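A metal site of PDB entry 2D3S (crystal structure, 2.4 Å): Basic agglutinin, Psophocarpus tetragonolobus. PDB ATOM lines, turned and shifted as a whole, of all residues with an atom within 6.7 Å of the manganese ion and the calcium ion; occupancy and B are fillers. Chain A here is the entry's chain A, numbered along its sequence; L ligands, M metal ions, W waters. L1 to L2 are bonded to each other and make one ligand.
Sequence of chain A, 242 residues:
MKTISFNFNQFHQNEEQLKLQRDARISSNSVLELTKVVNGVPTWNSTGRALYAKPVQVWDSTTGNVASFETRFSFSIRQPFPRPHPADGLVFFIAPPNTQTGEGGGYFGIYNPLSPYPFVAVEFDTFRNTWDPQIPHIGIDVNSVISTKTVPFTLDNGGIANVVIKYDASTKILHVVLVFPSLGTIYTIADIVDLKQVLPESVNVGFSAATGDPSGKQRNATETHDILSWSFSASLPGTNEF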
ATOM      1  N   ASP A  88      -8.811 -29.208  15.415  1.00  0.00           N
ATOM      2  CA  ASP A  88      -8.165 -28.093  16.108  1.00  0.00           C
ATOM      3  C   ASP A  88      -6.943 -27.544  15.362  1.00  0.00           C
ATOM      4  O   ASP A  88      -6.632 -26.352  15.441  1.00  0.00           O
ATOM      5  CB  ASP A  88      -7.730 -28.521  17.521  1.00  0.00           C
ATOM      6  CG  ASP A  88      -8.820 -28.292  18.544  1.00  0.00           C
ATOM      7  OD1 ASP A  88      -9.595 -29.236  18.827  1.00  0.00           O
ATOM      8  OD2 ASP A  88      -8.920 -27.156  19.056  1.00  0.00           O
ATOM      9  N   GLY A 105      -7.552 -31.622  21.777  1.00  0.00           N
ATOM     10  CA  GLY A 105      -8.148 -30.310  21.641  1.00  0.00           C
ATOM     11  C   GLY A 105      -7.132 -29.221  21.324  1.00  0.00           C
ATOM     12  O   GLY A 105      -6.180 -29.446  20.573  1.00  0.00           O
ATOM     13  N   GLY A 106      -7.341 -28.038  21.908  1.00  0.00           N
ATOM     14  CA  GLY A 106      -6.452 -26.917  21.674  1.00  0.00           C
ATOM     15  C   GLY A 106      -5.006 -27.135  22.060  1.00  0.00           C
ATOM     16  O   GLY A 106      -4.173 -26.248  21.863  1.00  0.00           O
ATOM     17  N   TYR A 107      -4.697 -28.291  22.637  1.00  0.00           N
ATOM     18  CA  TYR A 107      -3.315 -28.587  23.029  1.00  0.00           C
ATOM     19  C   TYR A 107      -2.599 -29.491  22.012  1.00  0.00           C
ATOM     20  O   TYR A 107      -1.460 -29.908  22.228  1.00  0.00           O
ATOM     21  CB  TYR A 107      -3.287 -29.221  24.418  1.00  0.00           C
ATOM     22  CG  TYR A 107      -3.750 -28.271  25.487  1.00  0.00           C
ATOM     23  CD1 TYR A 107      -3.012 -27.124  25.787  1.00  0.00           C
ATOM     24  CD2 TYR A 107      -4.942 -28.486  26.175  1.00  0.00           C
ATOM     25  CE1 TYR A 107      -3.454 -26.211  26.740  1.00  0.00           C
ATOM     26  CE2 TYR A 107      -5.405 -27.584  27.126  1.00  0.00           C
ATOM     27  CZ  TYR A 107      -4.660 -26.450  27.403  1.00  0.00           C
ATOM     28  OH  TYR A 107      -5.119 -25.554  28.342  1.00  0.00           O
ATOM     29  N   PHE A 108      -3.295 -29.769  20.917  1.00  0.00           N
ATOM     30  CA  PHE A 108      -2.772 -30.558  19.812  1.00  0.00           C
ATOM     31  C   PHE A 108      -2.204 -31.932  20.143  1.00  0.00           C
ATOM     32  O   PHE A 108      -1.737 -32.644  19.255  1.00  0.00           O
ATOM     33  CB  PHE A 108      -1.688 -29.740  19.095  1.00  0.00           C
ATOM     34  CG  PHE A 108      -2.103 -28.341  18.735  1.00  0.00           C
ATOM     35  CD1 PHE A 108      -3.128 -28.122  17.823  1.00  0.00           C
ATOM     36  CD2 PHE A 108      -1.427 -27.247  19.264  1.00  0.00           C
ATOM     37  CE1 PHE A 108      -3.464 -26.815  17.431  1.00  0.00           C
ATOM     38  CE2 PHE A 108      -1.757 -25.944  18.885  1.00  0.00           C
ATOM     39  CZ  PHE A 108      -2.778 -25.731  17.961  1.00  0.00           C
ATOM     40  N   GLU A 123       2.838 -24.452  14.865  1.00  0.00           N
ATOM     41  CA  GLU A 123       1.448 -24.824  14.727  1.00  0.00           C
ATOM     42  C   GLU A 123       0.713 -24.168  13.558  1.00  0.00           C
ATOM     43  O   GLU A 123       1.049 -23.062  13.110  1.00  0.00           O
ATOM     44  CB  GLU A 123       0.686 -24.478  16.016  1.00  0.00           C
ATOM     45  CG  GLU A 123       0.736 -22.992  16.332  1.00  0.00           C
ATOM     46  CD  GLU A 123      -0.185 -22.591  17.460  1.00  0.00           C
ATOM     47  OE1 GLU A 123      -0.078 -23.157  18.576  1.00  0.00           O
ATOM     48  OE2 GLU A 123      -1.004 -21.684  17.222  1.00  0.00           O
ATOM     49  N   ASP A 125      -2.875 -23.537  13.429  1.00  0.00           N
ATOM     50  CA  ASP A 125      -4.055 -23.481  14.257  1.00  0.00           C
ATOM     51  C   ASP A 125      -5.356 -23.099  13.565  1.00  0.00           C
ATOM     52  O   ASP A 125      -5.463 -22.027  12.977  1.00  0.00           O
ATOM     53  CB  ASP A 125      -3.783 -22.503  15.382  1.00  0.00           C
ATOM     54  CG  ASP A 125      -4.605 -22.787  16.598  1.00  0.00           C
ATOM     55  OD1 ASP A 125      -5.762 -23.233  16.455  1.00  0.00           O
ATOM     56  OD2 ASP A 125      -4.077 -22.558  17.698  1.00  0.00           O
ATOM     57  N   THR A 126      -6.360 -23.968  13.652  1.00  0.00           N
ATOM     58  CA  THR A 126      -7.643 -23.712  12.995  1.00  0.00           C
ATOM     59  C   THR A 126      -8.810 -23.358  13.914  1.00  0.00           C
ATOM     60  O   THR A 126      -9.900 -23.027  13.441  1.00  0.00           O
ATOM     61  CB  THR A 126      -8.049 -24.924  12.133  1.00  0.00           C
ATOM     62  OG1 THR A 126      -8.031 -26.103  12.955  1.00  0.00           O
ATOM     63  CG2 THR A 126      -7.081 -25.100  10.963  1.00  0.00           C
ATOM     64  N   PHE A 127      -8.596 -23.427  15.227  1.00  0.00           N
ATOM     65  CA  PHE A 127      -9.659 -23.121  16.173  1.00  0.00           C
ATOM     66  C   PHE A 127      -9.226 -22.058  17.179  1.00  0.00           C
ATOM     67  O   PHE A 127      -8.159 -22.153  17.764  1.00  0.00           O
ATOM     68  CB  PHE A 127     -10.086 -24.379  16.929  1.00  0.00           C
ATOM     69  CG  PHE A 127     -11.170 -24.116  17.944  1.00  0.00           C
ATOM     70  CD1 PHE A 127     -12.508 -24.050  17.553  1.00  0.00           C
ATOM     71  CD2 PHE A 127     -10.844 -23.887  19.288  1.00  0.00           C
ATOM     72  CE1 PHE A 127     -13.514 -23.748  18.488  1.00  0.00           C
ATOM     73  CE2 PHE A 127     -11.837 -23.583  20.218  1.00  0.00           C
ATOM     74  CZ  PHE A 127     -13.172 -23.504  19.821  1.00  0.00           C
ATOM     75  N   ARG A 128     -10.066 -21.057  17.405  1.00  0.00           N
ATOM     76  CA  ARG A 128      -9.694 -20.017  18.343  1.00  0.00           C
ATOM     77  C   ARG A 128      -9.962 -20.340  19.813  1.00  0.00           C
ATOM     78  O   ARG A 128     -11.095 -20.283  20.275  1.00  0.00           O
ATOM     79  CB  ARG A 128     -10.396 -18.711  17.979  1.00  0.00           C
ATOM     80  CG  ARG A 128      -9.789 -17.516  18.682  1.00  0.00           C
ATOM     81  CD  ARG A 128     -10.312 -16.221  18.106  1.00  0.00           C
ATOM     82  NE  ARG A 128      -9.582 -15.093  18.669  1.00  0.00           N
ATOM     83  CZ  ARG A 128      -9.845 -13.818  18.388  1.00  0.00           C
ATOM     84  NH1 ARG A 128     -10.825 -13.505  17.548  1.00  0.00           N
ATOM     85  NH2 ARG A 128      -9.118 -12.858  18.950  1.00  0.00           N
ATOM     86  N   ASN A 129      -8.919 -20.710  20.536  1.00  0.00           N
ATOM     87  CA  ASN A 129      -9.048 -21.003  21.960  1.00  0.00           C
ATOM     88  C   ASN A 129      -9.009 -19.667  22.686  1.00  0.00           C
ATOM     89  O   ASN A 129      -8.680 -18.646  22.072  1.00  0.00           O
ATOM     90  CB  ASN A 129      -7.914 -21.913  22.409  1.00  0.00           C
ATOM     91  CG  ASN A 129      -8.233 -23.379  22.236  1.00  0.00           C
ATOM     92  OD1 ASN A 129      -8.811 -24.025  23.130  1.00  0.00           O
ATOM     93  ND2 ASN A 129      -7.885 -23.928  21.080  1.00  0.00           N
ATOM     94  N   TRP A 131      -6.935 -18.372  24.399  1.00  0.00           N
ATOM     95  CA  TRP A 131      -5.600 -17.788  24.255  1.00  0.00           C
ATOM     96  C   TRP A 131      -5.116 -17.512  22.826  1.00  0.00           C
ATOM     97  O   TRP A 131      -3.936 -17.229  22.654  1.00  0.00           O
ATOM     98  CB  TRP A 131      -4.584 -18.707  24.922  1.00  0.00           C
ATOM     99  CG  TRP A 131      -4.486 -20.029  24.235  1.00  0.00           C
ATOM    100  CD1 TRP A 131      -3.883 -20.295  23.041  1.00  0.00           C
ATOM    101  CD2 TRP A 131      -5.058 -21.267  24.677  1.00  0.00           C
ATOM    102  NE1 TRP A 131      -4.048 -21.609  22.700  1.00  0.00           N
ATOM    103  CE2 TRP A 131      -4.768 -22.237  23.687  1.00  0.00           C
ATOM    104  CE3 TRP A 131      -5.800 -21.656  25.802  1.00  0.00           C
ATOM    105  CZ2 TRP A 131      -5.184 -23.563  23.792  1.00  0.00           C
ATOM    106  CZ3 TRP A 131      -6.207 -22.983  25.910  1.00  0.00           C
ATOM    107  CH2 TRP A 131      -5.897 -23.926  24.903  1.00  0.00           C
ATOM    108  N   ASP A 132      -5.982 -17.595  21.825  1.00  0.00           N
ATOM    109  CA  ASP A 132      -5.541 -17.347  20.448  1.00  0.00           C
ATOM    110  C   ASP A 132      -6.057 -16.097  19.815  1.00  0.00           C
ATOM    111  O   ASP A 132      -7.074 -15.538  20.230  1.00  0.00           O
ATOM    112  CB  ASP A 132      -5.983 -18.454  19.481  1.00  0.00           C
ATOM    113  CG  ASP A 132      -5.455 -19.805  19.837  1.00  0.00           C
ATOM    114  OD1 ASP A 132      -4.248 -19.945  20.081  1.00  0.00           O
ATOM    115  OD2 ASP A 132      -6.276 -20.731  19.857  1.00  0.00           O
ATOM    116  N   PRO A 133      -5.350 -15.629  18.770  1.00  0.00           N
ATOM    117  CA  PRO A 133      -5.723 -14.448  18.004  1.00  0.00           C
ATOM    118  C   PRO A 133      -6.575 -15.074  16.899  1.00  0.00           C
ATOM    119  O   PRO A 133      -6.832 -16.287  16.926  1.00  0.00           O
ATOM    120  CB  PRO A 133      -4.388 -13.935  17.485  1.00  0.00           C
ATOM    121  CG  PRO A 133      -3.627 -15.193  17.267  1.00  0.00           C
ATOM    122  CD  PRO A 133      -3.938 -15.985  18.520  1.00  0.00           C
ATOM    123  N   ILE A 135      -8.088 -17.028  13.903  1.00  0.00           N
ATOM    124  CA  ILE A 135      -7.633 -18.232  13.211  1.00  0.00           C
ATOM    125  C   ILE A 135      -8.131 -18.164  11.768  1.00  0.00           C
ATOM    126  O   ILE A 135      -9.069 -17.431  11.468  1.00  0.00           O
ATOM    127  CB  ILE A 135      -8.151 -19.530  13.916  1.00  0.00           C
ATOM    128  CG1 ILE A 135      -9.670 -19.457  14.154  1.00  0.00           C
ATOM    129  CG2 ILE A 135      -7.409 -19.737  15.224  1.00  0.00           C
ATOM    130  CD1 ILE A 135     -10.531 -19.705  12.908  1.00  0.00           C
ATOM    131  N   HIS A 137      -4.047 -19.475  11.881  1.00  0.00           N
ATOM    132  CA  HIS A 137      -2.787 -18.762  11.986  1.00  0.00           C
ATOM    133  C   HIS A 137      -1.643 -19.734  12.202  1.00  0.00           C
ATOM    134  O   HIS A 137      -1.842 -20.846  12.683  1.00  0.00           O
ATOM    135  CB  HIS A 137      -2.814 -17.733  13.116  1.00  0.00           C
ATOM    136  CG  HIS A 137      -3.102 -18.314  14.470  1.00  0.00           C
ATOM    137  ND1 HIS A 137      -4.340 -18.201  15.076  1.00  0.00           N
ATOM    138  CD2 HIS A 137      -2.327 -19.010  15.336  1.00  0.00           C
ATOM    139  CE1 HIS A 137      -4.303 -18.799  16.254  1.00  0.00           C
ATOM    140  NE2 HIS A 137      -3.094 -19.308  16.435  1.00  0.00           N
ATOM    141  N   ILE A 138      -0.451 -19.298  11.814  1.00  0.00           N
ATOM    142  CA  ILE A 138       0.765 -20.071  12.001  1.00  0.00           C
ATOM    143  C   ILE A 138       1.320 -19.524  13.297  1.00  0.00           C
ATOM    144  O   ILE A 138       1.187 -18.327  13.577  1.00  0.00           O
ATOM    145  CB  ILE A 138       1.798 -19.786  10.907  1.00  0.00           C
ATOM    146  CG1 ILE A 138       1.170 -19.961   9.523  1.00  0.00           C
ATOM    147  CG2 ILE A 138       2.981 -20.705  11.090  1.00  0.00           C
ATOM    148  CD1 ILE A 138       2.073 -19.510   8.384  1.00  0.00           C
ATOM    149  N   GLY A 139       1.924 -20.374  14.098  1.00  0.00           N
ATOM    150  CA  GLY A 139       2.460 -19.876  15.346  1.00  0.00           C
ATOM    151  C   GLY A 139       3.696 -20.626  15.765  1.00  0.00           C
ATOM    152  O   GLY A 139       3.850 -21.815  15.462  1.00  0.00           O
ATOM    153  N   ASP A 141       5.615 -21.948  18.887  1.00  0.00           N
ATOM    154  CA  ASP A 141       5.365 -22.298  20.276  1.00  0.00           C
ATOM    155  C   ASP A 141       6.587 -22.819  21.002  1.00  0.00           C
ATOM    156  O   ASP A 141       7.265 -23.726  20.524  1.00  0.00           O
ATOM    157  CB  ASP A 141       4.255 -23.352  20.372  1.00  0.00           C
ATOM    158  CG  ASP A 141       2.984 -22.931  19.695  1.00  0.00           C
ATOM    159  OD1 ASP A 141       2.845 -21.727  19.385  1.00  0.00           O
ATOM    160  OD2 ASP A 141       2.105 -23.791  19.464  1.00  0.00           O
ATOM    161  N   VAL A 145       1.431 -23.475  24.302  1.00  0.00           N
ATOM    162  CA  VAL A 145       0.599 -23.363  23.119  1.00  0.00           C
ATOM    163  C   VAL A 145       0.232 -21.890  22.927  1.00  0.00           C
ATOM    164  O   VAL A 145      -0.467 -21.514  21.988  1.00  0.00           O
ATOM    165  CB  VAL A 145      -0.666 -24.239  23.265  1.00  0.00           C
ATOM    166  CG1 VAL A 145      -1.759 -23.785  22.333  1.00  0.00           C
ATOM    167  CG2 VAL A 145      -0.305 -25.691  22.951  1.00  0.00           C
ATOM    168  N   ILE A 146       0.713 -21.050  23.846  1.00  0.00           N
ATOM    169  CA  ILE A 146       0.481 -19.620  23.742  1.00  0.00           C
ATOM    170  C   ILE A 146       1.700 -19.144  22.959  1.00  0.00           C
ATOM    171  O   ILE A 146       2.763 -18.886  23.522  1.00  0.00           O
ATOM    172  CB  ILE A 146       0.432 -18.972  25.146  1.00  0.00           C
ATOM    173  CG1 ILE A 146      -0.776 -19.525  25.909  1.00  0.00           C
ATOM    174  CG2 ILE A 146       0.364 -17.448  25.028  1.00  0.00           C
ATOM    175  CD1 ILE A 146      -0.834 -19.123  27.364  1.00  0.00           C
ATOM    176  N   SER A 147       1.517 -19.065  21.651  1.00  0.00           N
ATOM    177  CA  SER A 147       2.574 -18.692  20.709  1.00  0.00           C
ATOM    178  C   SER A 147       3.331 -17.409  21.017  1.00  0.00           C
ATOM    179  O   SER A 147       2.755 -16.403  21.423  1.00  0.00           O
ATOM    180  CB  SER A 147       1.991 -18.584  19.300  1.00  0.00           C
ATOM    181  OG  SER A 147       1.284 -19.763  18.969  1.00  0.00           O
ATOM    182  N   THR A 150       2.856 -14.949  15.995  1.00  0.00           N
ATOM    183  CA  THR A 150       1.744 -15.469  15.223  1.00  0.00           C
ATOM    184  C   THR A 150       1.504 -14.709  13.911  1.00  0.00           C
ATOM    185  O   THR A 150       1.775 -13.516  13.815  1.00  0.00           O
ATOM    186  CB  THR A 150       0.433 -15.426  16.081  1.00  0.00           C
ATOM    187  OG1 THR A 150       0.327 -16.617  16.858  1.00  0.00           O
ATOM    188  CG2 THR A 150      -0.791 -15.273  15.223  1.00  0.00           C
HETATM  189  N1  LIG L   1     -15.207 -23.692  23.506  1.00  0.00           N
HETATM  190  C1  LIG L   1     -14.560 -24.235  24.708  1.00  0.00           C
HETATM  191  C2  LIG L   1     -13.223 -23.527  25.002  1.00  0.00           C
HETATM  192  O1  LIG L   1     -12.502 -23.891  25.943  1.00  0.00           O
HETATM  193  C3  LIG L   1     -14.362 -25.753  24.520  1.00  0.00           C
HETATM  194  O2  LIG L   1     -13.400 -26.012  23.513  1.00  0.00           O
HETATM  195  O3  LIG L   1     -12.843 -22.569  24.297  1.00  0.00           O
HETATM  196  O1  LG2 L   2     -13.666 -27.942  22.213  1.00  0.00           O
HETATM  197  C1  LG2 L   2     -12.934 -27.350  23.314  1.00  0.00           C
HETATM  198  C2  LG2 L   2     -11.432 -27.306  23.006  1.00  0.00           C
HETATM  199  N1  LG2 L   2     -10.758 -26.681  24.128  1.00  0.00           N
HETATM  200  C3  LG2 L   2     -11.196 -26.530  21.694  1.00  0.00           C
HETATM  201  O2  LG2 L   2      -9.806 -26.484  21.397  1.00  0.00           O
HETATM  202  C4  LG2 L   2     -11.957 -27.218  20.561  1.00  0.00           C
HETATM  203  O3  LG2 L   2     -11.443 -28.538  20.411  1.00  0.00           O
HETATM  204  C5  LG2 L   2     -13.445 -27.263  20.943  1.00  0.00           C
HETATM  205  C6  LG2 L   2     -14.259 -27.959  19.864  1.00  0.00           C
HETATM  206  O4  LG2 L   2     -15.647 -27.752  20.155  1.00  0.00           O
HETATM  207  C7  LG2 L   2      -9.757 -27.265  24.797  1.00  0.00           C
HETATM  208  O5  LG2 L   2      -9.335 -28.370  24.487  1.00  0.00           O
HETATM  209  C8  LG2 L   2      -9.182 -26.469  25.933  1.00  0.00           C
HETATM  210 MN    MN M   1      -2.854 -20.679  18.328  1.00  0.00          MN
HETATM  211 CA    CA M   2      -6.275 -23.153  19.086  1.00  0.00          CA
HETATM  212  O   HOH W   1      -6.596 -25.814  18.509  1.00  0.00           O
HETATM  213  O   HOH W   2      -2.268 -22.007  19.951  1.00  0.00           O
HETATM  214  O   HOH W   3      -1.284 -19.330  19.247  1.00  0.00           O
HETATM  215  O   HOH W   4      -4.188 -24.043  20.382  1.00  0.00           O
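The side-chain carboxylate of Asp 88 is in hydrogen-bond range of an oxygen (O3) of LG2 L2, at 2.5 Å. OD1 of Asn 129 sits at hydrogen-bond distance from O2 of LG2 L2, 3.2 Å away. An oxygen (O2) of LG2 L2 sits at hydrogen-bond distance from the backbone NH of Gly 106 (3.0 Å).
NE of Arg 128 is in hydrogen-bond range of O of Asp 132. The backbone NH (N) of Glu 123 is in hydrogen-bond range of the backbone carbonyl oxygen (O) of Gly 139 (2.9 Å). The side-chain carboxylate (OD1) of Asp 132 lies close to the indole nitrogen (NE1) of Trp 131, 3.1 Å away. OE2 of Glu 123 sits close to OG of Ser 147, at 3.5 Å. The side-chain carboxylate of Glu 123 lies close to the side-chain carboxylate of Asp 141, at 2.4 Å.
Of the 23 residues printed, 4 come within 4 Å of the manganese ion. The nearest printed residue that does not touch the manganese ion is Ser 147 (4.3 Å).
Of the 23 residues printed, 4 come within 4 Å of the calcium ion.
Water W2 binds the manganese ion (2.2 Å). The manganese ion is bound by water W3 (2.3 Å). The manganese ion is bound by the side-chain carboxylate (OD2) of Asp 125 (2.3 Å). The manganese ion is bound by NE2 of His 137 (2.3 Å). The side-chain carboxylate (OD1) of Asp 132 is bound to the manganese ion (2.4 Å). The manganese ion is bound by the side-chain carboxylate (OE2) of Glu 123 (2.4 Å). The manganese ion has six donor atoms within binding distance.
The calcium ion is bound by O of Phe 127 (2.5 Å), OD2 of Asp 132 (2.5 Å), water W4 (2.6 Å), OD2 of Asp 125 (2.7 Å), ND2 of Asn 129 (2.7 Å), OD1 of Asp 125 (2.7 Å) and water W1 (2.7 Å). The calcium ion has seven donor atoms within binding distance.
Water W2 lies within hydrogen-bond range of O of Val 145, OE1 of Glu 123 and NE1 of Trp 131. Water W4 lies within hydrogen-bond range of O of Gly 106 (2.7 Å) and NE1 of Trp 131 (3.4 Å).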
